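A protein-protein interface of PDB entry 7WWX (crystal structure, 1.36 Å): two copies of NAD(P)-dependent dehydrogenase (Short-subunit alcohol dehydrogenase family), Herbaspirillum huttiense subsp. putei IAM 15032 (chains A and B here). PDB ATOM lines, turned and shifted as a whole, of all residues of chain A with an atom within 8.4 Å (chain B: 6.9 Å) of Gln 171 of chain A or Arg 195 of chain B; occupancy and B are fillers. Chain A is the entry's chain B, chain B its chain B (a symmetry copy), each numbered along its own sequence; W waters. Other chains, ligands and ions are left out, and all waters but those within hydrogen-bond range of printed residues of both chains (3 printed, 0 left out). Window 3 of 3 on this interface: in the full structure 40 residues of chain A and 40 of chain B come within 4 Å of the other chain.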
ATOM      1  N   ARG A 120      24.962  36.920  -8.907  1.00  0.00           N
ATOM      2  CA  ARG A 120      24.114  35.708  -9.032  1.00  0.00           C
ATOM      3  C   ARG A 120      22.641  36.111  -8.942  1.00  0.00           C
ATOM      4  O   ARG A 120      22.286  37.112  -8.259  1.00  0.00           O
ATOM      5  CB  ARG A 120      24.493  34.642  -8.005  1.00  0.00           C
ATOM      6  CG  ARG A 120      25.632  33.713  -8.423  1.00  0.00           C
ATOM      7  CD  ARG A 120      26.849  34.338  -9.027  1.00  0.00           C
ATOM      8  NE  ARG A 120      27.903  33.334  -9.211  1.00  0.00           N
ATOM      9  CZ  ARG A 120      29.137  33.597  -9.642  1.00  0.00           C
ATOM     10  NH1 ARG A 120      29.483  34.829  -9.998  1.00  0.00           N
ATOM     11  NH2 ARG A 120      30.029  32.614  -9.746  1.00  0.00           N
ATOM     12  N   SER A 166      33.159  34.584 -21.237  1.00  0.00           N
ATOM     13  CA  SER A 166      33.344  33.891 -19.954  1.00  0.00           C
ATOM     14  C   SER A 166      33.208  32.407 -20.192  1.00  0.00           C
ATOM     15  O   SER A 166      32.346  31.989 -20.985  1.00  0.00           O
ATOM     16  CB  SER A 166      32.299  34.332 -18.985  1.00  0.00           C
ATOM     17  OG  SER A 166      32.281  33.526 -17.813  1.00  0.00           O
ATOM     18  N   ILE A 167      33.948  31.587 -19.445  1.00  0.00           N
ATOM     19  CA  ILE A 167      33.686  30.129 -19.496  1.00  0.00           C
ATOM     20  C   ILE A 167      32.323  29.802 -18.891  1.00  0.00           C
ATOM     21  O   ILE A 167      31.878  28.684 -19.122  1.00  0.00           O
ATOM     22  CB  ILE A 167      34.785  29.266 -18.815  1.00  0.00           C
ATOM     23  CG1 ILE A 167      34.929  29.567 -17.324  1.00  0.00           C
ATOM     24  CG2 ILE A 167      36.083  29.339 -19.589  1.00  0.00           C
ATOM     25  CD1 ILE A 167      35.698  28.475 -16.511  1.00  0.00           C
ATOM     26  N   SER A 168      31.685  30.707 -18.170  1.00  0.00           N
ATOM     27  CA  SER A 168      30.371  30.411 -17.512  1.00  0.00           C
ATOM     28  C   SER A 168      29.394  29.757 -18.482  1.00  0.00           C
ATOM     29  O   SER A 168      28.754  28.782 -18.111  1.00  0.00           O
ATOM     30  CB  SER A 168      29.748  31.629 -16.906  1.00  0.00           C
ATOM     31  OG  SER A 168      29.604  32.648 -17.901  1.00  0.00           O
ATOM     32  N   TRP A 169      29.248  30.274 -19.692  1.00  0.00           N
ATOM     33  CA  TRP A 169      28.235  29.733 -20.624  1.00  0.00           C
ATOM     34  C   TRP A 169      28.721  28.413 -21.220  1.00  0.00           C
ATOM     35  O   TRP A 169      27.950  27.485 -21.420  1.00  0.00           O
ATOM     36  CB  TRP A 169      27.839  30.769 -21.669  1.00  0.00           C
ATOM     37  CG  TRP A 169      28.810  31.080 -22.740  1.00  0.00           C
ATOM     38  CD1 TRP A 169      29.759  32.062 -22.757  1.00  0.00           C
ATOM     39  CD2 TRP A 169      28.898  30.419 -24.000  1.00  0.00           C
ATOM     40  NE1 TRP A 169      30.427  32.035 -23.946  1.00  0.00           N
ATOM     41  CE2 TRP A 169      29.927  31.041 -24.736  1.00  0.00           C
ATOM     42  CE3 TRP A 169      28.182  29.365 -24.592  1.00  0.00           C
ATOM     43  CZ2 TRP A 169      30.285  30.637 -26.010  1.00  0.00           C
ATOM     44  CZ3 TRP A 169      28.515  28.991 -25.864  1.00  0.00           C
ATOM     45  CH2 TRP A 169      29.516  29.638 -26.570  1.00  0.00           C
ATOM     46  N   HIS A 170      30.015  28.304 -21.452  1.00  0.00           N
ATOM     47  CA  HIS A 170      30.639  27.060 -21.907  1.00  0.00           C
ATOM     48  C   HIS A 170      30.490  25.946 -20.879  1.00  0.00           C
ATOM     49  O   HIS A 170      30.351  24.791 -21.323  1.00  0.00           O
ATOM     50  CB  HIS A 170      32.137  27.264 -22.197  1.00  0.00           C
ATOM     51  CG  HIS A 170      32.465  28.111 -23.387  1.00  0.00           C
ATOM     52  ND1 HIS A 170      32.388  27.622 -24.689  1.00  0.00           N
ATOM     53  CD2 HIS A 170      33.016  29.332 -23.495  1.00  0.00           C
ATOM     54  CE1 HIS A 170      32.789  28.573 -25.543  1.00  0.00           C
ATOM     55  NE2 HIS A 170      33.235  29.594 -24.824  1.00  0.00           N
ATOM     56  N   GLN A 171      30.484  26.265 -19.593  1.00  0.00           N
ATOM     57  CA  GLN A 171      30.341  25.313 -18.457  1.00  0.00           C
ATOM     58  C   GLN A 171      28.869  24.934 -18.247  1.00  0.00           C
ATOM     59  O   GLN A 171      28.619  24.108 -17.331  1.00  0.00           O
ATOM     60  CB  GLN A 171      30.720  26.005 -17.140  1.00  0.00           C
ATOM     61  CG  GLN A 171      32.184  26.288 -16.888  1.00  0.00           C
ATOM     62  CD  GLN A 171      32.247  27.048 -15.580  1.00  0.00           C
ATOM     63  OE1 GLN A 171      32.040  28.248 -15.530  1.00  0.00           O
ATOM     64  NE2 GLN A 171      32.391  26.339 -14.478  1.00  0.00           N
ATOM     65  N   SER A 172      27.920  25.558 -18.931  1.00  0.00           N
ATOM     66  CA  SER A 172      26.496  25.526 -18.502  1.00  0.00           C
ATOM     67  C   SER A 172      26.448  25.904 -17.026  1.00  0.00           C
ATOM     68  O   SER A 172      25.866  25.220 -16.196  1.00  0.00           O
ATOM     69  CB  SER A 172      25.830  24.206 -18.784  1.00  0.00           C
ATOM     70  OG  SER A 172      25.877  23.987 -20.199  1.00  0.00           O
ATOM     71  N   GLY A 173      27.036  27.047 -16.688  1.00  0.00           N
ATOM     72  CA  GLY A 173      27.110  27.442 -15.287  1.00  0.00           C
ATOM     73  C   GLY A 173      25.755  27.885 -14.759  1.00  0.00           C
ATOM     74  O   GLY A 173      25.049  28.689 -15.401  1.00  0.00           O
ATOM     75  N   GLY A 174      25.390  27.356 -13.587  1.00  0.00           N
ATOM     76  CA  GLY A 174      24.115  27.684 -12.961  1.00  0.00           C
ATOM     77  C   GLY A 174      24.220  28.947 -12.139  1.00  0.00           C
ATOM     78  O   GLY A 174      25.347  29.460 -11.879  1.00  0.00           O
ATOM     79  N   GLY A 175      23.056  29.411 -11.741  1.00  0.00           N
ATOM     80  CA  GLY A 175      22.940  30.488 -10.738  1.00  0.00           C
ATOM     81  C   GLY A 175      22.996  31.886 -11.305  1.00  0.00           C
ATOM     82  O   GLY A 175      23.024  32.817 -10.494  1.00  0.00           O
ATOM     83  N   PHE A 176      23.011  32.127 -12.623  1.00  0.00           N
ATOM     84  CA  PHE A 176      23.012  33.494 -13.191  1.00  0.00           C
ATOM     85  C   PHE A 176      22.650  33.487 -14.671  1.00  0.00           C
ATOM     86  O   PHE A 176      23.470  33.862 -15.519  1.00  0.00           O
ATOM     87  CB  PHE A 176      24.325  34.235 -12.937  1.00  0.00           C
ATOM     88  CG  PHE A 176      25.639  33.555 -13.207  1.00  0.00           C
ATOM     89  CD1 PHE A 176      25.754  32.376 -13.939  1.00  0.00           C
ATOM     90  CD2 PHE A 176      26.781  34.134 -12.719  1.00  0.00           C
ATOM     91  CE1 PHE A 176      27.007  31.822 -14.188  1.00  0.00           C
ATOM     92  CE2 PHE A 176      28.028  33.584 -12.953  1.00  0.00           C
ATOM     93  CZ  PHE A 176      28.130  32.415 -13.666  1.00  0.00           C
ATOM     94  N   TYR A 179      23.375  36.491 -16.899  1.00  0.00           N
ATOM     95  CA  TYR A 179      24.833  36.682 -17.102  1.00  0.00           C
ATOM     96  C   TYR A 179      25.335  35.718 -18.185  1.00  0.00           C
ATOM     97  O   TYR A 179      26.084  36.164 -19.100  1.00  0.00           O
ATOM     98  CB  TYR A 179      25.570  36.428 -15.800  1.00  0.00           C
ATOM     99  CG  TYR A 179      27.050  36.656 -15.879  1.00  0.00           C
ATOM    100  CD1 TYR A 179      27.615  37.912 -16.018  1.00  0.00           C
ATOM    101  CD2 TYR A 179      27.874  35.559 -15.845  1.00  0.00           C
ATOM    102  CE1 TYR A 179      28.990  38.078 -16.084  1.00  0.00           C
ATOM    103  CE2 TYR A 179      29.245  35.710 -15.818  1.00  0.00           C
ATOM    104  CZ  TYR A 179      29.807  36.970 -15.972  1.00  0.00           C
ATOM    105  OH  TYR A 179      31.203  37.034 -16.014  1.00  0.00           O
ATOM    106  N   THR A 180      24.982  34.435 -18.112  1.00  0.00           N
ATOM    107  CA  THR A 180      25.405  33.492 -19.160  1.00  0.00           C
ATOM    108  C   THR A 180      24.854  33.996 -20.482  1.00  0.00           C
ATOM    109  O   THR A 180      25.543  33.846 -21.522  1.00  0.00           O
ATOM    110  CB  THR A 180      25.021  32.047 -18.838  1.00  0.00           C
ATOM    111  OG1 THR A 180      23.613  31.912 -18.604  1.00  0.00           O
ATOM    112  CG2 THR A 180      25.770  31.540 -17.623  1.00  0.00           C
ATOM    113  N   THR A 208      38.070  34.796 -23.609  1.00  0.00           N
ATOM    114  CA  THR A 208      37.211  34.040 -22.662  1.00  0.00           C
ATOM    115  C   THR A 208      38.033  33.541 -21.506  1.00  0.00           C
ATOM    116  O   THR A 208      38.758  32.570 -21.638  1.00  0.00           O
ATOM    117  CB  THR A 208      36.549  32.894 -23.413  1.00  0.00           C
ATOM    118  OG1 THR A 208      35.747  33.496 -24.424  1.00  0.00           O
ATOM    119  CG2 THR A 208      35.735  32.028 -22.497  1.00  0.00           C
ATOM    120  N   PRO A 209      37.962  34.239 -20.361  1.00  0.00           N
ATOM    121  CA  PRO A 209      38.652  33.763 -19.175  1.00  0.00           C
ATOM    122  C   PRO A 209      37.990  32.549 -18.524  1.00  0.00           C
ATOM    123  O   PRO A 209      36.795  32.397 -18.551  1.00  0.00           O
ATOM    124  CB  PRO A 209      38.627  34.925 -18.223  1.00  0.00           C
ATOM    125  CG  PRO A 209      38.169  36.103 -19.047  1.00  0.00           C
ATOM    126  CD  PRO A 209      37.315  35.518 -20.137  1.00  0.00           C
ATOM    127  N   GLY A 210      38.832  31.742 -17.915  1.00  0.00           N
ATOM    128  CA  GLY A 210      38.474  30.752 -16.893  1.00  0.00           C
ATOM    129  C   GLY A 210      38.147  31.439 -15.587  1.00  0.00           C
ATOM    130  O   GLY A 210      37.760  32.618 -15.529  1.00  0.00           O
ATOM    131  N   TRP A 211      38.279  30.710 -14.496  1.00  0.00           N
ATOM    132  CA  TRP A 211      37.954  31.256 -13.177  1.00  0.00           C
ATOM    133  C   TRP A 211      39.166  31.989 -12.626  1.00  0.00           C
ATOM    134  O   TRP A 211      40.099  31.404 -12.091  1.00  0.00           O
ATOM    135  CB  TRP A 211      37.431  30.199 -12.235  1.00  0.00           C
ATOM    136  CG  TRP A 211      36.657  30.836 -11.108  1.00  0.00           C
ATOM    137  CD1 TRP A 211      36.318  32.162 -10.966  1.00  0.00           C
ATOM    138  CD2 TRP A 211      36.046  30.168  -9.992  1.00  0.00           C
ATOM    139  NE1 TRP A 211      35.604  32.355  -9.801  1.00  0.00           N
ATOM    140  CE2 TRP A 211      35.427  31.150  -9.193  1.00  0.00           C
ATOM    141  CE3 TRP A 211      35.983  28.829  -9.596  1.00  0.00           C
ATOM    142  CZ2 TRP A 211      34.715  30.833  -8.035  1.00  0.00           C
ATOM    143  CZ3 TRP A 211      35.327  28.510  -8.425  1.00  0.00           C
ATOM    144  CH2 TRP A 211      34.704  29.505  -7.660  1.00  0.00           C
ATOM    145  N   ALA A 229      36.464  22.360  -6.949  1.00  0.00           N
ATOM    146  CA  ALA A 229      35.983  22.428  -8.338  1.00  0.00           C
ATOM    147  C   ALA A 229      37.122  22.943  -9.214  1.00  0.00           C
ATOM    148  O   ALA A 229      37.280  22.395 -10.298  1.00  0.00           O
ATOM    149  CB  ALA A 229      34.776  23.322  -8.438  1.00  0.00           C
ATOM    150  N   ILE A 230      37.853  23.954  -8.781  1.00  0.00           N
ATOM    151  CA  ILE A 230      38.975  24.484  -9.611  1.00  0.00           C
ATOM    152  C   ILE A 230      40.003  23.371  -9.816  1.00  0.00           C
ATOM    153  O   ILE A 230      40.485  23.133 -10.943  1.00  0.00           O
ATOM    154  CB  ILE A 230      39.595  25.725  -8.950  1.00  0.00           C
ATOM    155  CG1 ILE A 230      38.606  26.883  -9.035  1.00  0.00           C
ATOM    156  CG2 ILE A 230      40.941  26.047  -9.582  1.00  0.00           C
ATOM    157  CD1 ILE A 230      38.934  28.089  -8.131  1.00  0.00           C
ATOM    158  N   ASN A 233      38.749  20.610 -12.199  1.00  0.00           N
ATOM    159  CA  ASN A 233      38.418  20.989 -13.580  1.00  0.00           C
ATOM    160  C   ASN A 233      39.592  21.573 -14.340  1.00  0.00           C
ATOM    161  O   ASN A 233      39.677  21.358 -15.554  1.00  0.00           O
ATOM    162  CB  ASN A 233      37.260  21.946 -13.617  1.00  0.00           C
ATOM    163  CG  ASN A 233      35.949  21.224 -13.412  1.00  0.00           C
ATOM    164  OD1 ASN A 233      35.516  20.466 -14.275  1.00  0.00           O
ATOM    165  ND2 ASN A 233      35.415  21.348 -12.194  1.00  0.00           N
ATOM    166  N   ASP A 268      42.087  29.629 -19.713  1.00  0.00           N
ATOM    167  CA  ASP A 268      41.232  29.012 -18.685  1.00  0.00           C
ATOM    168  C   ASP A 268      41.923  27.867 -17.964  1.00  0.00           C
ATOM    169  O   ASP A 268      41.208  27.151 -17.238  1.00  0.00           O
ATOM    170  CB  ASP A 268      39.905  28.570 -19.265  1.00  0.00           C
ATOM    171  CG  ASP A 268      39.974  27.283 -20.028  1.00  0.00           C
ATOM    172  OD1 ASP A 268      41.077  26.951 -20.532  1.00  0.00           O
ATOM    173  OD2 ASP A 268      38.909  26.631 -20.162  1.00  0.00           O
ATOM    174  N   TRP A 271      39.921  24.281 -18.297  1.00  0.00           N
ATOM    175  CA  TRP A 271      38.593  23.946 -17.725  1.00  0.00           C
ATOM    176  C   TRP A 271      37.637  23.435 -18.823  1.00  0.00           C
ATOM    177  O   TRP A 271      36.987  22.378 -18.643  1.00  0.00           O
ATOM    178  CB  TRP A 271      38.044  25.184 -17.016  1.00  0.00           C
ATOM    179  CG  TRP A 271      36.932  24.869 -16.060  1.00  0.00           C
ATOM    180  CD1 TRP A 271      35.804  24.142 -16.270  1.00  0.00           C
ATOM    181  CD2 TRP A 271      36.842  25.340 -14.702  1.00  0.00           C
ATOM    182  NE1 TRP A 271      35.026  24.140 -15.161  1.00  0.00           N
ATOM    183  CE2 TRP A 271      35.650  24.821 -14.159  1.00  0.00           C
ATOM    184  CE3 TRP A 271      37.696  26.046 -13.868  1.00  0.00           C
ATOM    185  CZ2 TRP A 271      35.285  24.989 -12.815  1.00  0.00           C
ATOM    186  CZ3 TRP A 271      37.310  26.271 -12.564  1.00  0.00           C
ATOM    187  CH2 TRP A 271      36.139  25.714 -12.036  1.00  0.00           C
ATOM    188  N   VAL A 272      37.423  24.217 -19.893  1.00  0.00           N
ATOM    189  CA  VAL A 272      36.295  23.901 -20.812  1.00  0.00           C
ATOM    190  C   VAL A 272      36.826  23.417 -22.149  1.00  0.00           C
ATOM    191  O   VAL A 272      38.002  23.277 -22.318  1.00  0.00           O
ATOM    192  CB  VAL A 272      35.319  25.081 -21.041  1.00  0.00           C
ATOM    193  CG1 VAL A 272      34.711  25.536 -19.719  1.00  0.00           C
ATOM    194  CG2 VAL A 272      35.966  26.266 -21.776  1.00  0.00           C
ATOM    195  OXT VAL A 272      35.972  23.174 -23.062  1.00  0.00           O
ATOM    196  N   THR B 190      20.243  29.070 -22.981  1.00  0.00           N
ATOM    197  CA  THR B 190      20.024  27.617 -22.999  1.00  0.00           C
ATOM    198  C   THR B 190      20.907  26.985 -21.930  1.00  0.00           C
ATOM    199  O   THR B 190      20.437  26.133 -21.138  1.00  0.00           O
ATOM    200  CB  THR B 190      20.331  27.008 -24.378  1.00  0.00           C
ATOM    201  OG1 THR B 190      19.299  27.420 -25.272  1.00  0.00           O
ATOM    202  CG2 THR B 190      20.408  25.504 -24.313  1.00  0.00           C
ATOM    203  N   ARG B 191      22.205  27.273 -21.957  1.00  0.00           N
ATOM    204  CA  ARG B 191      23.147  26.491 -21.124  1.00  0.00           C
ATOM    205  C   ARG B 191      23.037  26.876 -19.666  1.00  0.00           C
ATOM    206  O   ARG B 191      23.026  25.920 -18.847  1.00  0.00           O
ATOM    207  CB  ARG B 191      24.542  26.616 -21.729  1.00  0.00           C
ATOM    208  CG  ARG B 191      24.570  25.911 -23.081  1.00  0.00           C
ATOM    209  CD  ARG B 191      25.854  26.006 -23.828  1.00  0.00           C
ATOM    210  NE  ARG B 191      26.970  25.333 -23.201  1.00  0.00           N
ATOM    211  CZ  ARG B 191      27.234  24.025 -23.327  1.00  0.00           C
ATOM    212  NH1 ARG B 191      28.359  23.554 -22.816  1.00  0.00           N
ATOM    213  NH2 ARG B 191      26.415  23.209 -23.973  1.00  0.00           N
ATOM    214  N   GLY B 192      22.802  28.162 -19.361  1.00  0.00           N
ATOM    215  CA  GLY B 192      22.600  28.520 -17.937  1.00  0.00           C
ATOM    216  C   GLY B 192      21.324  27.852 -17.439  1.00  0.00           C
ATOM    217  O   GLY B 192      21.284  27.211 -16.329  1.00  0.00           O
ATOM    218  N   LEU B 193      20.277  27.885 -18.207  1.00  0.00           N
ATOM    219  CA  LEU B 193      19.003  27.298 -17.726  1.00  0.00           C
ATOM    220  C   LEU B 193      19.063  25.780 -17.734  1.00  0.00           C
ATOM    221  O   LEU B 193      18.363  25.150 -16.887  1.00  0.00           O
ATOM    222  CB  LEU B 193      17.852  27.753 -18.597  1.00  0.00           C
ATOM    223  CG  LEU B 193      17.472  29.221 -18.489  1.00  0.00           C
ATOM    224  CD1 LEU B 193      16.415  29.538 -19.548  1.00  0.00           C
ATOM    225  CD2 LEU B 193      17.002  29.561 -17.067  1.00  0.00           C
ATOM    226  N   ALA B 194      19.812  25.137 -18.612  1.00  0.00           N
ATOM    227  CA  ALA B 194      19.864  23.658 -18.586  1.00  0.00           C
ATOM    228  C   ALA B 194      20.336  23.195 -17.215  1.00  0.00           C
ATOM    229  O   ALA B 194      19.815  22.206 -16.641  1.00  0.00           O
ATOM    230  CB  ALA B 194      20.769  23.154 -19.681  1.00  0.00           C
ATOM    231  N   ARG B 195      21.307  23.904 -16.651  1.00  0.00           N
ATOM    232  CA  ARG B 195      21.839  23.550 -15.338  1.00  0.00           C
ATOM    233  C   ARG B 195      20.817  23.853 -14.227  1.00  0.00           C
ATOM    234  O   ARG B 195      20.621  22.985 -13.347  1.00  0.00           O
ATOM    235  CB  ARG B 195      23.128  24.346 -15.148  1.00  0.00           C
ATOM    236  CG  ARG B 195      23.833  23.974 -13.859  1.00  0.00           C
ATOM    237  CD  ARG B 195      24.609  22.649 -13.931  1.00  0.00           C
ATOM    238  NE  ARG B 195      25.693  22.663 -14.941  1.00  0.00           N
ATOM    239  CZ  ARG B 195      26.367  21.613 -15.359  1.00  0.00           C
ATOM    240  NH1 ARG B 195      26.135  20.405 -14.855  1.00  0.00           N
ATOM    241  NH2 ARG B 195      27.257  21.705 -16.328  1.00  0.00           N
ATOM    242  N   ASP B 196      20.194  25.009 -14.312  1.00  0.00           N
ATOM    243  CA  ASP B 196      19.259  25.485 -13.241  1.00  0.00           C
ATOM    244  C   ASP B 196      17.980  24.625 -13.244  1.00  0.00           C
ATOM    245  O   ASP B 196      17.407  24.354 -12.134  1.00  0.00           O
ATOM    246  CB  ASP B 196      18.933  26.966 -13.452  1.00  0.00           C
ATOM    247  CG  ASP B 196      20.064  27.976 -13.281  1.00  0.00           C
ATOM    248  OD1 ASP B 196      21.052  27.669 -12.605  1.00  0.00           O
ATOM    249  OD2 ASP B 196      19.937  29.089 -13.907  1.00  0.00           O
ATOM    250  N   LEU B 197      17.520  24.154 -14.395  1.00  0.00           N
ATOM    251  CA  LEU B 197      16.202  23.493 -14.518  1.00  0.00           C
ATOM    252  C   LEU B 197      16.327  21.991 -14.627  1.00  0.00           C
ATOM    253  O   LEU B 197      15.294  21.283 -14.492  1.00  0.00           O
ATOM    254  CB  LEU B 197      15.465  24.098 -15.717  1.00  0.00           C
ATOM    255  CG  LEU B 197      15.231  25.605 -15.651  1.00  0.00           C
ATOM    256  CD1 LEU B 197      14.420  26.127 -16.829  1.00  0.00           C
ATOM    257  CD2 LEU B 197      14.538  25.947 -14.304  1.00  0.00           C
ATOM    258  N   GLY B 198      17.517  21.485 -14.917  1.00  0.00           N
ATOM    259  CA  GLY B 198      17.689  20.025 -15.040  1.00  0.00           C
ATOM    260  C   GLY B 198      17.218  19.217 -13.819  1.00  0.00           C
ATOM    261  O   GLY B 198      16.673  18.127 -14.003  1.00  0.00           O
ATOM    262  N   PRO B 199      17.418  19.722 -12.580  1.00  0.00           N
ATOM    263  CA  PRO B 199      16.898  19.001 -11.409  1.00  0.00           C
ATOM    264  C   PRO B 199      15.385  18.784 -11.431  1.00  0.00           C
ATOM    265  O   PRO B 199      14.899  17.893 -10.715  1.00  0.00           O
ATOM    266  CB  PRO B 199      17.281  19.925 -10.242  1.00  0.00           C
ATOM    267  CG  PRO B 199      18.521  20.630 -10.745  1.00  0.00           C
ATOM    268  CD  PRO B 199      18.227  20.885 -12.216  1.00  0.00           C
ATOM    269  N   ILE B 202      13.531  19.313 -16.566  1.00  0.00           N
ATOM    270  CA  ILE B 202      13.247  20.225 -17.695  1.00  0.00           C
ATOM    271  C   ILE B 202      14.500  20.297 -18.564  1.00  0.00           C
ATOM    272  O   ILE B 202      15.543  20.702 -18.072  1.00  0.00           O
ATOM    273  CB  ILE B 202      12.849  21.606 -17.194  1.00  0.00           C
ATOM    274  CG1 ILE B 202      11.562  21.544 -16.356  1.00  0.00           C
ATOM    275  CG2 ILE B 202      12.763  22.586 -18.357  1.00  0.00           C
ATOM    276  CD1 ILE B 202      11.288  22.835 -15.592  1.00  0.00           C
ATOM    277  N   VAL B 204      16.537  21.812 -21.834  1.00  0.00           N
ATOM    278  CA  VAL B 204      16.681  23.112 -22.515  1.00  0.00           C
ATOM    279  C   VAL B 204      17.724  22.932 -23.623  1.00  0.00           C
ATOM    280  O   VAL B 204      18.857  22.605 -23.312  1.00  0.00           O
ATOM    281  CB  VAL B 204      17.083  24.248 -21.567  1.00  0.00           C
ATOM    282  CG1 VAL B 204      16.863  25.583 -22.253  1.00  0.00           C
ATOM    283  CG2 VAL B 204      16.337  24.188 -20.246  1.00  0.00           C
ATOM    284  N   THR B 261      20.030  17.678 -23.334  1.00  0.00           N
ATOM    285  CA  THR B 261      19.914  19.020 -22.716  1.00  0.00           C
ATOM    286  C   THR B 261      21.254  19.746 -22.892  1.00  0.00           C
ATOM    287  O   THR B 261      22.299  19.107 -23.012  1.00  0.00           O
ATOM    288  CB  THR B 261      19.374  18.966 -21.280  1.00  0.00           C
ATOM    289  OG1 THR B 261      18.874  20.253 -20.935  1.00  0.00           O
ATOM    290  CG2 THR B 261      20.459  18.591 -20.303  1.00  0.00           C
ATOM    291  N   ALA B 262      21.132  21.070 -22.950  1.00  0.00           N
ATOM    292  CA  ALA B 262      22.203  22.085 -22.995  1.00  0.00           C
ATOM    293  C   ALA B 262      22.764  22.263 -24.409  1.00  0.00           C
ATOM    294  O   ALA B 262      23.593  23.149 -24.583  1.00  0.00           O
ATOM    295  CB  ALA B 262      23.316  21.798 -21.986  1.00  0.00           C
HETATM  296  O   HOH W   1      22.719  30.261 -14.880  1.00  0.00           O
HETATM  297  O   HOH W   2      27.016  21.481 -20.350  1.00  0.00           O
HETATM  298  O   HOH W   3      30.696  22.102 -16.703  1.00  0.00           O
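O of His 170 of chain A is in hydrogen-bond range of NH1 of Arg 191 of chain B, 2.8 Å away. NE of Arg 191 of chain B sits close to OG of Ser 172 of chain A (3.5 Å). NE of Arg 195 of chain B lies within hydrogen-bond range of O of Ser 172 of chain A, at 2.9 Å. NH2 of Arg 195 of chain B sits at hydrogen-bond distance from O of Gln 171 of chain A (2.9 Å). The backbone NH (N) of Gly 175 of chain A lies within hydrogen-bond range of the side-chain carboxylate (OD1) of Asp 196 of chain B, 2.8 Å away. O of Trp 169 of chain A lies within hydrogen-bond range of NE of Arg 191 of chain B (3.0 Å).
O of Val 204 of chain B sits at hydrogen-bond distance from N of Ala 262 of chain B, at 2.8 Å. The guanidinium group of Arg 191 of chain B lies within hydrogen-bond range of the backbone carbonyl oxygen of Ala 262 of chain B, at 2.9 Å. The indole nitrogen (NE1) of Trp 271 of chain A sits close to the side-chain amide nitrogen (NE2) of Gln 171 of chain A. O of Ser 168 of chain A lies within hydrogen-bond range of N of Gly 173 of chain A (2.8 Å).
CB of Ala 262 of chain B touches OG of Ser 172 of chain A, at 3.8 Å. Gly 173 of chain A touches Gly 192 of chain B (O to CA, 3.5 Å). Arg 195 of chain B touches Gly 174 of chain A (CG to N, 3.7 Å). OD1 of Asp 196 of chain B touches CA of Gly 174 of chain A (3.1 Å). Gly 192 of chain B touches Thr 180 of chain A.
Of chain B, only Arg 195 comes within 4 Å of Gln 171 of chain A. Arg 195 of chain B touches three residues of chain A. No residue of chain A comes within 4 Å of Ala 194 of chain B. Of the printed residues of chain B, Trp 169 of chain A touches Arg 191 (3.0 Å). Printed residues of chain A within 4 Å of Ala 262 of chain B: Ser 172. Printed residues of chain A within 4 Å of Arg 191 of chain B: Trp 169 (3.0 Å), His 170 (2.8 Å) and Ser 172 (3.3 Å). Printed residues of chain B within 4 Å of Gly 174 of chain A: Arg 195 (3.7 Å) and Asp 196 (3.1 Å). Gly 198 of chain B touches none of the printed residues of chain A. Asn 233 of chain A touches none of the printed residues of chain B. The nearest residue of chain A that does not touch Arg 195 of chain B is Gly 173 of chain A (4.4 Å).
Of the 24 printed residues of chain A, 8 touch a printed residue of chain B. Of the 14 printed residues of chain B, 5 touch a printed residue of chain A. Hydrophobic or aromatic side chains of chain B within 4 Å of the printed part of chain A: Ala 262.
No position is printed for both chains. Of the 11 pairs that touch across the chains among the printed residues, none has its exchanged pair printed and touching as well.
Water W2 bridges the side-chain hydroxyl (OG) of Ser 172 of chain A (2.8 Å) and the guanidinium group (NH1) of Arg 191 of chain B (3.5 Å). Water W1 lies within hydrogen-bond range of the backbone carbonyl oxygen (O) of Gly 173 of chain A (2.9 Å), the backbone NH (N) of Phe 176 of chain A (2.9 Å), the side-chain carboxylate (OD2) of Asp 196 of chain B (3.2 Å) and the backbone NH (N) of Gly 175 of chain A (3.3 Å). Water W3 lies within hydrogen-bond range of the backbone carbonyl oxygen of Gln 171 of chain A (3.0 Å) and the guanidinium group of Arg 195 of chain B (3.5 Å).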
